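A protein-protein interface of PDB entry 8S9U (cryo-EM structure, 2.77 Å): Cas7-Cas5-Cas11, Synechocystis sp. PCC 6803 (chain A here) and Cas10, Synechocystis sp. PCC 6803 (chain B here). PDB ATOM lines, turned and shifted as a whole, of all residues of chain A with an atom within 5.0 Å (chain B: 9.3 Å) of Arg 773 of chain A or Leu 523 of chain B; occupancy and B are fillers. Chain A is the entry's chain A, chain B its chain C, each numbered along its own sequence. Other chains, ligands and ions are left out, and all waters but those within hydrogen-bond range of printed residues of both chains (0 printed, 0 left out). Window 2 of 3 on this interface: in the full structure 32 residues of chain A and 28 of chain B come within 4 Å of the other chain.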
ATOM      1  N   LEU A 645     -11.845 -20.276  21.552  1.00  0.00           N
ATOM      2  CA  LEU A 645     -10.672 -20.008  22.380  1.00  0.00           C
ATOM      3  C   LEU A 645      -9.382 -20.379  21.670  1.00  0.00           C
ATOM      4  O   LEU A 645      -8.436 -19.588  21.625  1.00  0.00           O
ATOM      5  CB  LEU A 645     -10.767 -20.786  23.692  1.00  0.00           C
ATOM      6  CG  LEU A 645     -11.144 -20.160  25.029  1.00  0.00           C
ATOM      7  CD1 LEU A 645     -11.489 -21.263  25.990  1.00  0.00           C
ATOM      8  CD2 LEU A 645      -9.986 -19.371  25.582  1.00  0.00           C
ATOM      9  N   ARG A 769     -10.928 -10.664  22.233  1.00  0.00           N
ATOM     10  CA  ARG A 769     -10.271 -10.795  23.528  1.00  0.00           C
ATOM     11  C   ARG A 769      -8.828 -11.260  23.387  1.00  0.00           C
ATOM     12  O   ARG A 769      -7.928 -10.713  24.029  1.00  0.00           O
ATOM     13  CB  ARG A 769     -11.055 -11.745  24.427  1.00  0.00           C
ATOM     14  CG  ARG A 769     -10.530 -11.804  25.849  1.00  0.00           C
ATOM     15  CD  ARG A 769     -11.345 -12.733  26.724  1.00  0.00           C
ATOM     16  NE  ARG A 769     -12.713 -12.263  26.876  1.00  0.00           N
ATOM     17  CZ  ARG A 769     -13.755 -12.714  26.193  1.00  0.00           C
ATOM     18  NH1 ARG A 769     -13.678 -13.853  25.528  1.00  0.00           N
ATOM     19  NH2 ARG A 769     -14.942 -12.167  26.395  1.00  0.00           N
ATOM     20  N   GLY A 770      -8.587 -12.284  22.569  1.00  0.00           N
ATOM     21  CA  GLY A 770      -7.227 -12.742  22.342  1.00  0.00           C
ATOM     22  C   GLY A 770      -6.361 -11.716  21.644  1.00  0.00           C
ATOM     23  O   GLY A 770      -5.155 -11.656  21.876  1.00  0.00           O
ATOM     24  N   HIS A 771      -6.963 -10.910  20.774  1.00  0.00           N
ATOM     25  CA  HIS A 771      -6.268  -9.781  20.171  1.00  0.00           C
ATOM     26  C   HIS A 771      -5.829  -8.762  21.210  1.00  0.00           C
ATOM     27  O   HIS A 771      -4.660  -8.373  21.255  1.00  0.00           O
ATOM     28  CB  HIS A 771      -7.183  -9.122  19.150  1.00  0.00           C
ATOM     29  CG  HIS A 771      -6.606  -7.902  18.509  1.00  0.00           C
ATOM     30  ND1 HIS A 771      -5.348  -7.869  17.954  1.00  0.00           N
ATOM     31  CD2 HIS A 771      -7.121  -6.664  18.343  1.00  0.00           C
ATOM     32  CE1 HIS A 771      -5.121  -6.667  17.460  1.00  0.00           C
ATOM     33  NE2 HIS A 771      -6.178  -5.914  17.689  1.00  0.00           N
ATOM     34  N   LYS A 772      -6.756  -8.318  22.057  1.00  0.00           N
ATOM     35  CA  LYS A 772      -6.421  -7.296  23.038  1.00  0.00           C
ATOM     36  C   LYS A 772      -5.376  -7.783  24.024  1.00  0.00           C
ATOM     37  O   LYS A 772      -4.515  -7.012  24.456  1.00  0.00           O
ATOM     38  CB  LYS A 772      -7.670  -6.847  23.781  1.00  0.00           C
ATOM     39  CG  LYS A 772      -7.593  -5.404  24.224  1.00  0.00           C
ATOM     40  CD  LYS A 772      -6.997  -5.241  25.594  1.00  0.00           C
ATOM     41  CE  LYS A 772      -6.714  -3.782  25.879  1.00  0.00           C
ATOM     42  NZ  LYS A 772      -6.368  -3.574  27.307  1.00  0.00           N
ATOM     43  N   ARG A 773      -5.442  -9.049  24.408  1.00  0.00           N
ATOM     44  CA  ARG A 773      -4.473  -9.592  25.347  1.00  0.00           C
ATOM     45  C   ARG A 773      -3.146  -9.967  24.708  1.00  0.00           C
ATOM     46  O   ARG A 773      -2.157 -10.122  25.429  1.00  0.00           O
ATOM     47  CB  ARG A 773      -5.108 -10.758  26.086  1.00  0.00           C
ATOM     48  CG  ARG A 773      -6.310 -10.252  26.844  1.00  0.00           C
ATOM     49  CD  ARG A 773      -6.669 -11.083  28.028  1.00  0.00           C
ATOM     50  NE  ARG A 773      -7.950 -10.666  28.577  1.00  0.00           N
ATOM     51  CZ  ARG A 773      -8.375 -10.985  29.790  1.00  0.00           C
ATOM     52  NH1 ARG A 773      -9.535 -10.528  30.228  1.00  0.00           N
ATOM     53  NH2 ARG A 773      -7.629 -11.747  30.571  1.00  0.00           N
ATOM     54  N   ASP A 774      -3.092 -10.125  23.387  1.00  0.00           N
ATOM     55  CA  ASP A 774      -1.799 -10.116  22.715  1.00  0.00           C
ATOM     56  C   ASP A 774      -1.303  -8.702  22.476  1.00  0.00           C
ATOM     57  O   ASP A 774      -0.093  -8.463  22.495  1.00  0.00           O
ATOM     58  CB  ASP A 774      -1.879 -10.848  21.376  1.00  0.00           C
ATOM     59  CG  ASP A 774      -1.789 -12.353  21.516  1.00  0.00           C
ATOM     60  OD1 ASP A 774      -1.469 -12.845  22.621  1.00  0.00           O
ATOM     61  OD2 ASP A 774      -2.035 -13.049  20.508  1.00  0.00           O
ATOM     62  N   LEU A 775      -2.217  -7.765  22.232  1.00  0.00           N
ATOM     63  CA  LEU A 775      -1.853  -6.356  22.164  1.00  0.00           C
ATOM     64  C   LEU A 775      -1.244  -5.855  23.465  1.00  0.00           C
ATOM     65  O   LEU A 775      -0.241  -5.139  23.446  1.00  0.00           O
ATOM     66  CB  LEU A 775      -3.079  -5.527  21.799  1.00  0.00           C
ATOM     67  CG  LEU A 775      -2.915  -4.019  21.721  1.00  0.00           C
ATOM     68  CD1 LEU A 775      -1.956  -3.647  20.630  1.00  0.00           C
ATOM     69  CD2 LEU A 775      -4.256  -3.402  21.470  1.00  0.00           C
ATOM     70  N   GLU A 776      -1.832  -6.219  24.606  1.00  0.00           N
ATOM     71  CA  GLU A 776      -1.234  -5.890  25.898  1.00  0.00           C
ATOM     72  C   GLU A 776       0.198  -6.391  26.045  1.00  0.00           C
ATOM     73  O   GLU A 776       1.013  -5.724  26.685  1.00  0.00           O
ATOM     74  CB  GLU A 776      -2.093  -6.448  27.027  1.00  0.00           C
ATOM     75  CG  GLU A 776      -3.363  -5.673  27.284  1.00  0.00           C
ATOM     76  CD  GLU A 776      -4.273  -6.378  28.264  1.00  0.00           C
ATOM     77  OE1 GLU A 776      -5.401  -5.898  28.492  1.00  0.00           O
ATOM     78  OE2 GLU A 776      -3.851  -7.410  28.821  1.00  0.00           O
ATOM     79  N   LYS A 777       0.537  -7.549  25.480  1.00  0.00           N
ATOM     80  CA  LYS A 777       1.924  -7.992  25.568  1.00  0.00           C
ATOM     81  C   LYS A 777       2.849  -7.144  24.709  1.00  0.00           C
ATOM     82  O   LYS A 777       4.010  -6.941  25.070  1.00  0.00           O
ATOM     83  CB  LYS A 777       2.063  -9.458  25.167  1.00  0.00           C
ATOM     84  CG  LYS A 777       1.284 -10.439  26.001  1.00  0.00           C
ATOM     85  CD  LYS A 777       1.594 -11.855  25.554  1.00  0.00           C
ATOM     86  CE  LYS A 777       0.731 -12.884  26.257  1.00  0.00           C
ATOM     87  NZ  LYS A 777      -0.647 -12.910  25.715  1.00  0.00           N
ATOM     88  N   GLN B 502      -8.211 -16.091  39.403  1.00  0.00           N
ATOM     89  CA  GLN B 502      -7.503 -16.460  38.184  1.00  0.00           C
ATOM     90  C   GLN B 502      -6.875 -17.845  38.236  1.00  0.00           C
ATOM     91  O   GLN B 502      -6.775 -18.504  37.198  1.00  0.00           O
ATOM     92  CB  GLN B 502      -6.405 -15.438  37.883  1.00  0.00           C
ATOM     93  CG  GLN B 502      -6.869 -14.002  37.778  1.00  0.00           C
ATOM     94  CD  GLN B 502      -7.946 -13.786  36.742  1.00  0.00           C
ATOM     95  OE1 GLN B 502      -8.022 -14.497  35.748  1.00  0.00           O
ATOM     96  NE2 GLN B 502      -8.778 -12.787  36.963  1.00  0.00           N
ATOM     97  N   ALA B 505      -9.740 -19.991  37.149  1.00  0.00           N
ATOM     98  CA  ALA B 505      -9.900 -19.923  35.701  1.00  0.00           C
ATOM     99  C   ALA B 505      -8.944 -20.884  35.008  1.00  0.00           C
ATOM    100  O   ALA B 505      -9.329 -21.599  34.078  1.00  0.00           O
ATOM    101  CB  ALA B 505      -9.677 -18.494  35.216  1.00  0.00           C
ATOM    102  N   LEU B 506      -7.684 -20.894  35.438  1.00  0.00           N
ATOM    103  CA  LEU B 506      -6.701 -21.822  34.890  1.00  0.00           C
ATOM    104  C   LEU B 506      -7.034 -23.268  35.237  1.00  0.00           C
ATOM    105  O   LEU B 506      -6.942 -24.157  34.387  1.00  0.00           O
ATOM    106  CB  LEU B 506      -5.311 -21.460  35.405  1.00  0.00           C
ATOM    107  CG  LEU B 506      -4.728 -20.134  34.933  1.00  0.00           C
ATOM    108  CD1 LEU B 506      -3.444 -19.840  35.676  1.00  0.00           C
ATOM    109  CD2 LEU B 506      -4.498 -20.154  33.441  1.00  0.00           C
ATOM    110  N   ALA B 509      -9.606 -24.441  32.907  1.00  0.00           N
ATOM    111  CA  ALA B 509      -9.040 -24.646  31.577  1.00  0.00           C
ATOM    112  C   ALA B 509      -8.226 -25.926  31.467  1.00  0.00           C
ATOM    113  O   ALA B 509      -8.137 -26.505  30.381  1.00  0.00           O
ATOM    114  CB  ALA B 509      -8.170 -23.458  31.197  1.00  0.00           C
ATOM    115  N   ASN B 515      -4.575 -27.046  23.812  1.00  0.00           N
ATOM    116  CA  ASN B 515      -4.762 -25.844  23.004  1.00  0.00           C
ATOM    117  C   ASN B 515      -5.721 -24.859  23.652  1.00  0.00           C
ATOM    118  O   ASN B 515      -5.628 -23.652  23.407  1.00  0.00           O
ATOM    119  CB  ASN B 515      -5.265 -26.218  21.614  1.00  0.00           C
ATOM    120  CG  ASN B 515      -4.288 -27.076  20.860  1.00  0.00           C
ATOM    121  OD1 ASN B 515      -3.222 -27.418  21.373  1.00  0.00           O
ATOM    122  ND2 ASN B 515      -4.637 -27.428  19.629  1.00  0.00           N
ATOM    123  N   GLU B 516      -6.645 -25.342  24.471  1.00  0.00           N
ATOM    124  CA  GLU B 516      -7.546 -24.456  25.192  1.00  0.00           C
ATOM    125  C   GLU B 516      -7.014 -24.082  26.563  1.00  0.00           C
ATOM    126  O   GLU B 516      -7.288 -22.980  27.045  1.00  0.00           O
ATOM    127  CB  GLU B 516      -8.920 -25.108  25.326  1.00  0.00           C
ATOM    128  CG  GLU B 516      -9.658 -25.234  24.015  1.00  0.00           C
ATOM    129  CD  GLU B 516      -9.765 -26.668  23.539  1.00  0.00           C
ATOM    130  OE1 GLU B 516      -9.539 -26.912  22.336  1.00  0.00           O
ATOM    131  OE2 GLU B 516     -10.058 -27.555  24.366  1.00  0.00           O
ATOM    132  N   ALA B 517      -6.286 -24.987  27.211  1.00  0.00           N
ATOM    133  CA  ALA B 517      -5.611 -24.635  28.453  1.00  0.00           C
ATOM    134  C   ALA B 517      -4.547 -23.576  28.210  1.00  0.00           C
ATOM    135  O   ALA B 517      -4.445 -22.596  28.955  1.00  0.00           O
ATOM    136  CB  ALA B 517      -4.993 -25.884  29.081  1.00  0.00           C
ATOM    137  N   ASP B 518      -3.743 -23.762  27.161  1.00  0.00           N
ATOM    138  CA  ASP B 518      -2.758 -22.766  26.756  1.00  0.00           C
ATOM    139  C   ASP B 518      -3.390 -21.471  26.271  1.00  0.00           C
ATOM    140  O   ASP B 518      -2.792 -20.404  26.426  1.00  0.00           O
ATOM    141  CB  ASP B 518      -1.868 -23.349  25.669  1.00  0.00           C
ATOM    142  CG  ASP B 518      -1.039 -24.503  26.163  1.00  0.00           C
ATOM    143  OD1 ASP B 518      -1.113 -24.825  27.364  1.00  0.00           O
ATOM    144  OD2 ASP B 518      -0.306 -25.092  25.348  1.00  0.00           O
ATOM    145  N   ALA B 519      -4.572 -21.537  25.666  1.00  0.00           N
ATOM    146  CA  ALA B 519      -5.276 -20.319  25.279  1.00  0.00           C
ATOM    147  C   ALA B 519      -5.652 -19.484  26.495  1.00  0.00           C
ATOM    148  O   ALA B 519      -5.405 -18.276  26.530  1.00  0.00           O
ATOM    149  CB  ALA B 519      -6.513 -20.669  24.458  1.00  0.00           C
ATOM    150  N   GLN B 520      -6.272 -20.112  27.494  1.00  0.00           N
ATOM    151  CA  GLN B 520      -6.588 -19.428  28.744  1.00  0.00           C
ATOM    152  C   GLN B 520      -5.348 -18.852  29.408  1.00  0.00           C
ATOM    153  O   GLN B 520      -5.355 -17.707  29.869  1.00  0.00           O
ATOM    154  CB  GLN B 520      -7.285 -20.389  29.703  1.00  0.00           C
ATOM    155  CG  GLN B 520      -8.788 -20.338  29.669  1.00  0.00           C
ATOM    156  CD  GLN B 520      -9.334 -19.363  30.681  1.00  0.00           C
ATOM    157  OE1 GLN B 520      -8.584 -18.604  31.292  1.00  0.00           O
ATOM    158  NE2 GLN B 520     -10.645 -19.375  30.865  1.00  0.00           N
ATOM    159  N   TYR B 521      -4.278 -19.641  29.487  1.00  0.00           N
ATOM    160  CA  TYR B 521      -3.038 -19.153  30.080  1.00  0.00           C
ATOM    161  C   TYR B 521      -2.483 -17.957  29.317  1.00  0.00           C
ATOM    162  O   TYR B 521      -1.967 -17.014  29.924  1.00  0.00           O
ATOM    163  CB  TYR B 521      -2.031 -20.295  30.155  1.00  0.00           C
ATOM    164  CG  TYR B 521      -0.699 -19.941  30.762  1.00  0.00           C
ATOM    165  CD1 TYR B 521       0.335 -19.452  29.991  1.00  0.00           C
ATOM    166  CD2 TYR B 521      -0.487 -20.081  32.120  1.00  0.00           C
ATOM    167  CE1 TYR B 521       1.546 -19.127  30.557  1.00  0.00           C
ATOM    168  CE2 TYR B 521       0.718 -19.764  32.687  1.00  0.00           C
ATOM    169  CZ  TYR B 521       1.728 -19.287  31.904  1.00  0.00           C
ATOM    170  OH  TYR B 521       2.938 -18.981  32.475  1.00  0.00           O
ATOM    171  N   SER B 522      -2.571 -17.972  27.989  1.00  0.00           N
ATOM    172  CA  SER B 522      -2.108 -16.835  27.205  1.00  0.00           C
ATOM    173  C   SER B 522      -2.973 -15.593  27.393  1.00  0.00           C
ATOM    174  O   SER B 522      -2.505 -14.484  27.125  1.00  0.00           O
ATOM    175  CB  SER B 522      -2.065 -17.207  25.726  1.00  0.00           C
ATOM    176  OG  SER B 522      -1.209 -18.312  25.515  1.00  0.00           O
ATOM    177  N   LEU B 523      -4.213 -15.748  27.846  1.00  0.00           N
ATOM    178  CA  LEU B 523      -5.032 -14.610  28.239  1.00  0.00           C
ATOM    179  C   LEU B 523      -4.624 -14.018  29.577  1.00  0.00           C
ATOM    180  O   LEU B 523      -5.143 -12.966  29.959  1.00  0.00           O
ATOM    181  CB  LEU B 523      -6.504 -15.015  28.291  1.00  0.00           C
ATOM    182  CG  LEU B 523      -7.392 -14.677  27.099  1.00  0.00           C
ATOM    183  CD1 LEU B 523      -6.765 -15.128  25.811  1.00  0.00           C
ATOM    184  CD2 LEU B 523      -8.736 -15.323  27.284  1.00  0.00           C
ATOM    185  N   ILE B 524      -3.710 -14.664  30.294  1.00  0.00           N
ATOM    186  CA  ILE B 524      -3.439 -14.342  31.691  1.00  0.00           C
ATOM    187  C   ILE B 524      -1.957 -14.149  31.963  1.00  0.00           C
ATOM    188  O   ILE B 524      -1.594 -13.438  32.914  1.00  0.00           O
ATOM    189  CB  ILE B 524      -4.022 -15.445  32.605  1.00  0.00           C
ATOM    190  CG1 ILE B 524      -5.519 -15.606  32.379  1.00  0.00           C
ATOM    191  CG2 ILE B 524      -3.880 -15.105  34.050  1.00  0.00           C
ATOM    192  CD1 ILE B 524      -6.109 -16.776  33.134  1.00  0.00           C
ATOM    193  N   SER B 525      -1.077 -14.722  31.142  1.00  0.00           N
ATOM    194  CA  SER B 525       0.327 -14.893  31.491  1.00  0.00           C
ATOM    195  C   SER B 525       1.041 -13.578  31.786  1.00  0.00           C
ATOM    196  O   SER B 525       1.980 -13.558  32.587  1.00  0.00           O
ATOM    197  CB  SER B 525       1.040 -15.640  30.369  1.00  0.00           C
ATOM    198  OG  SER B 525       1.062 -14.868  29.185  1.00  0.00           O
ATOM    199  N   GLN B 526       0.632 -12.478  31.158  1.00  0.00           N
ATOM    200  CA  GLN B 526       1.315 -11.205  31.352  1.00  0.00           C
ATOM    201  C   GLN B 526       0.529 -10.222  32.203  1.00  0.00           C
ATOM    202  O   GLN B 526       1.036  -9.135  32.490  1.00  0.00           O
ATOM    203  CB  GLN B 526       1.628 -10.558  29.998  1.00  0.00           C
ATOM    204  CG  GLN B 526       2.698 -11.273  29.181  1.00  0.00           C
ATOM    205  CD  GLN B 526       4.037 -10.559  29.202  1.00  0.00           C
ATOM    206  OE1 GLN B 526       5.009 -11.056  29.766  1.00  0.00           O
ATOM    207  NE2 GLN B 526       4.092  -9.386  28.588  1.00  0.00           N
ATOM    208  N   ARG B 527      -0.692 -10.564  32.606  1.00  0.00           N
ATOM    209  CA  ARG B 527      -1.367  -9.842  33.674  1.00  0.00           C
ATOM    210  C   ARG B 527      -0.863 -10.210  35.061  1.00  0.00           C
ATOM    211  O   ARG B 527      -1.023  -9.412  35.988  1.00  0.00           O
ATOM    212  CB  ARG B 527      -2.869 -10.090  33.588  1.00  0.00           C
ATOM    213  CG  ARG B 527      -3.535  -9.395  32.435  1.00  0.00           C
ATOM    214  CD  ARG B 527      -5.032  -9.517  32.530  1.00  0.00           C
ATOM    215  NE  ARG B 527      -5.702  -8.677  31.553  1.00  0.00           N
ATOM    216  CZ  ARG B 527      -6.897  -8.133  31.734  1.00  0.00           C
ATOM    217  NH1 ARG B 527      -7.626  -8.471  32.783  1.00  0.00           N
ATOM    218  NH2 ARG B 527      -7.421  -7.361  30.794  1.00  0.00           N
ATOM    219  N   TYR B 528      -0.264 -11.392  35.230  1.00  0.00           N
ATOM    220  CA  TYR B 528       0.172 -11.870  36.547  1.00  0.00           C
ATOM    221  C   TYR B 528       1.552 -12.502  36.393  1.00  0.00           C
ATOM    222  O   TYR B 528       1.670 -13.686  36.075  1.00  0.00           O
ATOM    223  CB  TYR B 528      -0.835 -12.849  37.141  1.00  0.00           C
ATOM    224  CG  TYR B 528      -2.234 -12.294  37.172  1.00  0.00           C
ATOM    225  CD1 TYR B 528      -2.645 -11.442  38.176  1.00  0.00           C
ATOM    226  CD2 TYR B 528      -3.138 -12.613  36.181  1.00  0.00           C
ATOM    227  CE1 TYR B 528      -3.913 -10.930  38.187  1.00  0.00           C
ATOM    228  CE2 TYR B 528      -4.403 -12.109  36.187  1.00  0.00           C
ATOM    229  CZ  TYR B 528      -4.788 -11.267  37.187  1.00  0.00           C
ATOM    230  OH  TYR B 528      -6.059 -10.763  37.189  1.00  0.00           O
ATOM    231  N   LEU B 531       3.022 -15.992  37.153  1.00  0.00           N
ATOM    232  CA  LEU B 531       2.750 -17.142  36.296  1.00  0.00           C
ATOM    233  C   LEU B 531       3.945 -17.578  35.462  1.00  0.00           C
ATOM    234  O   LEU B 531       3.931 -18.690  34.926  1.00  0.00           O
ATOM    235  CB  LEU B 531       1.574 -16.848  35.372  1.00  0.00           C
ATOM    236  CG  LEU B 531       0.211 -16.830  36.046  1.00  0.00           C
ATOM    237  CD1 LEU B 531      -0.830 -16.447  35.043  1.00  0.00           C
ATOM    238  CD2 LEU B 531      -0.078 -18.196  36.622  1.00  0.00           C
ATOM    239  N   ASN B 540       7.205 -20.154  28.844  1.00  0.00           N
ATOM    240  CA  ASN B 540       6.357 -19.236  29.604  1.00  0.00           C
ATOM    241  C   ASN B 540       5.063 -18.943  28.855  1.00  0.00           C
ATOM    242  O   ASN B 540       4.574 -17.815  28.848  1.00  0.00           O
ATOM    243  CB  ASN B 540       7.088 -17.941  29.968  1.00  0.00           C
ATOM    244  CG  ASN B 540       8.378 -18.195  30.726  1.00  0.00           C
ATOM    245  OD1 ASN B 540       8.719 -19.338  31.029  1.00  0.00           O
ATOM    246  ND2 ASN B 540       9.101 -17.125  31.040  1.00  0.00           N
ATOM    247  N   LYS B 541       4.509 -19.976  28.220  1.00  0.00           N
ATOM    248  CA  LYS B 541       3.225 -19.873  27.546  1.00  0.00           C
ATOM    249  C   LYS B 541       2.313 -21.072  27.774  1.00  0.00           C
ATOM    250  O   LYS B 541       1.204 -21.085  27.231  1.00  0.00           O
ATOM    251  CB  LYS B 541       3.425 -19.647  26.039  1.00  0.00           C
ATOM    252  CG  LYS B 541       4.241 -20.701  25.336  1.00  0.00           C
ATOM    253  CD  LYS B 541       4.342 -20.373  23.863  1.00  0.00           C
ATOM    254  CE  LYS B 541       5.085 -19.065  23.650  1.00  0.00           C
ATOM    255  NZ  LYS B 541       5.333 -18.795  22.208  1.00  0.00           N
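The side-chain amino group (NZ) of Lys 777 of chain A sits at hydrogen-bond distance from the backbone carbonyl oxygen (O) of Arg 773 of chain A, at 3.2 Å. The backbone carbonyl oxygen (O) of Asp 518 of chain B is in hydrogen-bond range of the side-chain hydroxyl (OG) of Ser 522 of chain B (2.8 Å). The side-chain carboxylate of Glu 776 of chain A lies within salt-bridge range of the side-chain amino group of Lys 772 of chain A (2.8 Å). The side-chain amino group (NZ) of Lys 777 of chain A is in salt-bridge range of the side-chain carboxylate (OD1) of Asp 774 of chain A.
Printed residues of chain A that touch a printed residue of chain B: Leu 645, Arg 769, Arg 773, Glu 776 and Lys 777. Hydrophobic or aromatic side chains of chain A within 4 Å of the printed part of chain B: Leu 645. Of the 21 printed residues of chain B, 6 touch a printed residue of chain A. Hydrophobic or aromatic side chains of chain B that line the printed part of chain A: Ala 519 and Leu 523. Along chain B the printed residues that touch a printed residue of chain A span positions 519 to 527.
Arg 773 of chain A touches just these residues of chain B: Leu 523 (2.8 Å) and Arg 527 (3.8 Å). Leu 523 of chain B touches two residues of chain A. No residue of chain B comes within 4 Å of Gly 770 of chain A. Printed residues of chain A within 4 Å of Ala 519 of chain B: Leu 645 (3.6 Å). Of the printed residues of chain B, Arg 769 of chain A touches Leu 523. Of the printed residues of chain B, Glu 776 of chain A touches Arg 527 (3.4 Å). Of the printed residues of chain B, Lys 777 of chain A touches Ser 522 (2.8 Å), Ser 525 (3.6 Å) and Gln 526 (3.6 Å). The nearest residue of chain A that does not touch Leu 523 of chain B is Gly 770 of chain A (4.2 Å).
OE1 of Glu 776 of chain A is in salt-bridge range of NH2 of Arg 527 of chain B. The backbone carbonyl oxygen (O) of Leu 523 of chain B lies within hydrogen-bond range of the guanidinium group (NH2) of Arg 773 of chain A. NZ of Lys 777 of chain A sits at hydrogen-bond distance from O of Ser 522 of chain B (2.8 Å).
Among the printed residues, merely in contact across the chains: Lys 777 of chain A with Ser 525 of chain B, Lys 777 of chain A with Gln 526 of chain B, Leu 645 of chain A with Ala 519 of chain B, Arg 769 of chain A with Leu 523 of chain B and Arg 773 of chain A with Arg 527 of chain B.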
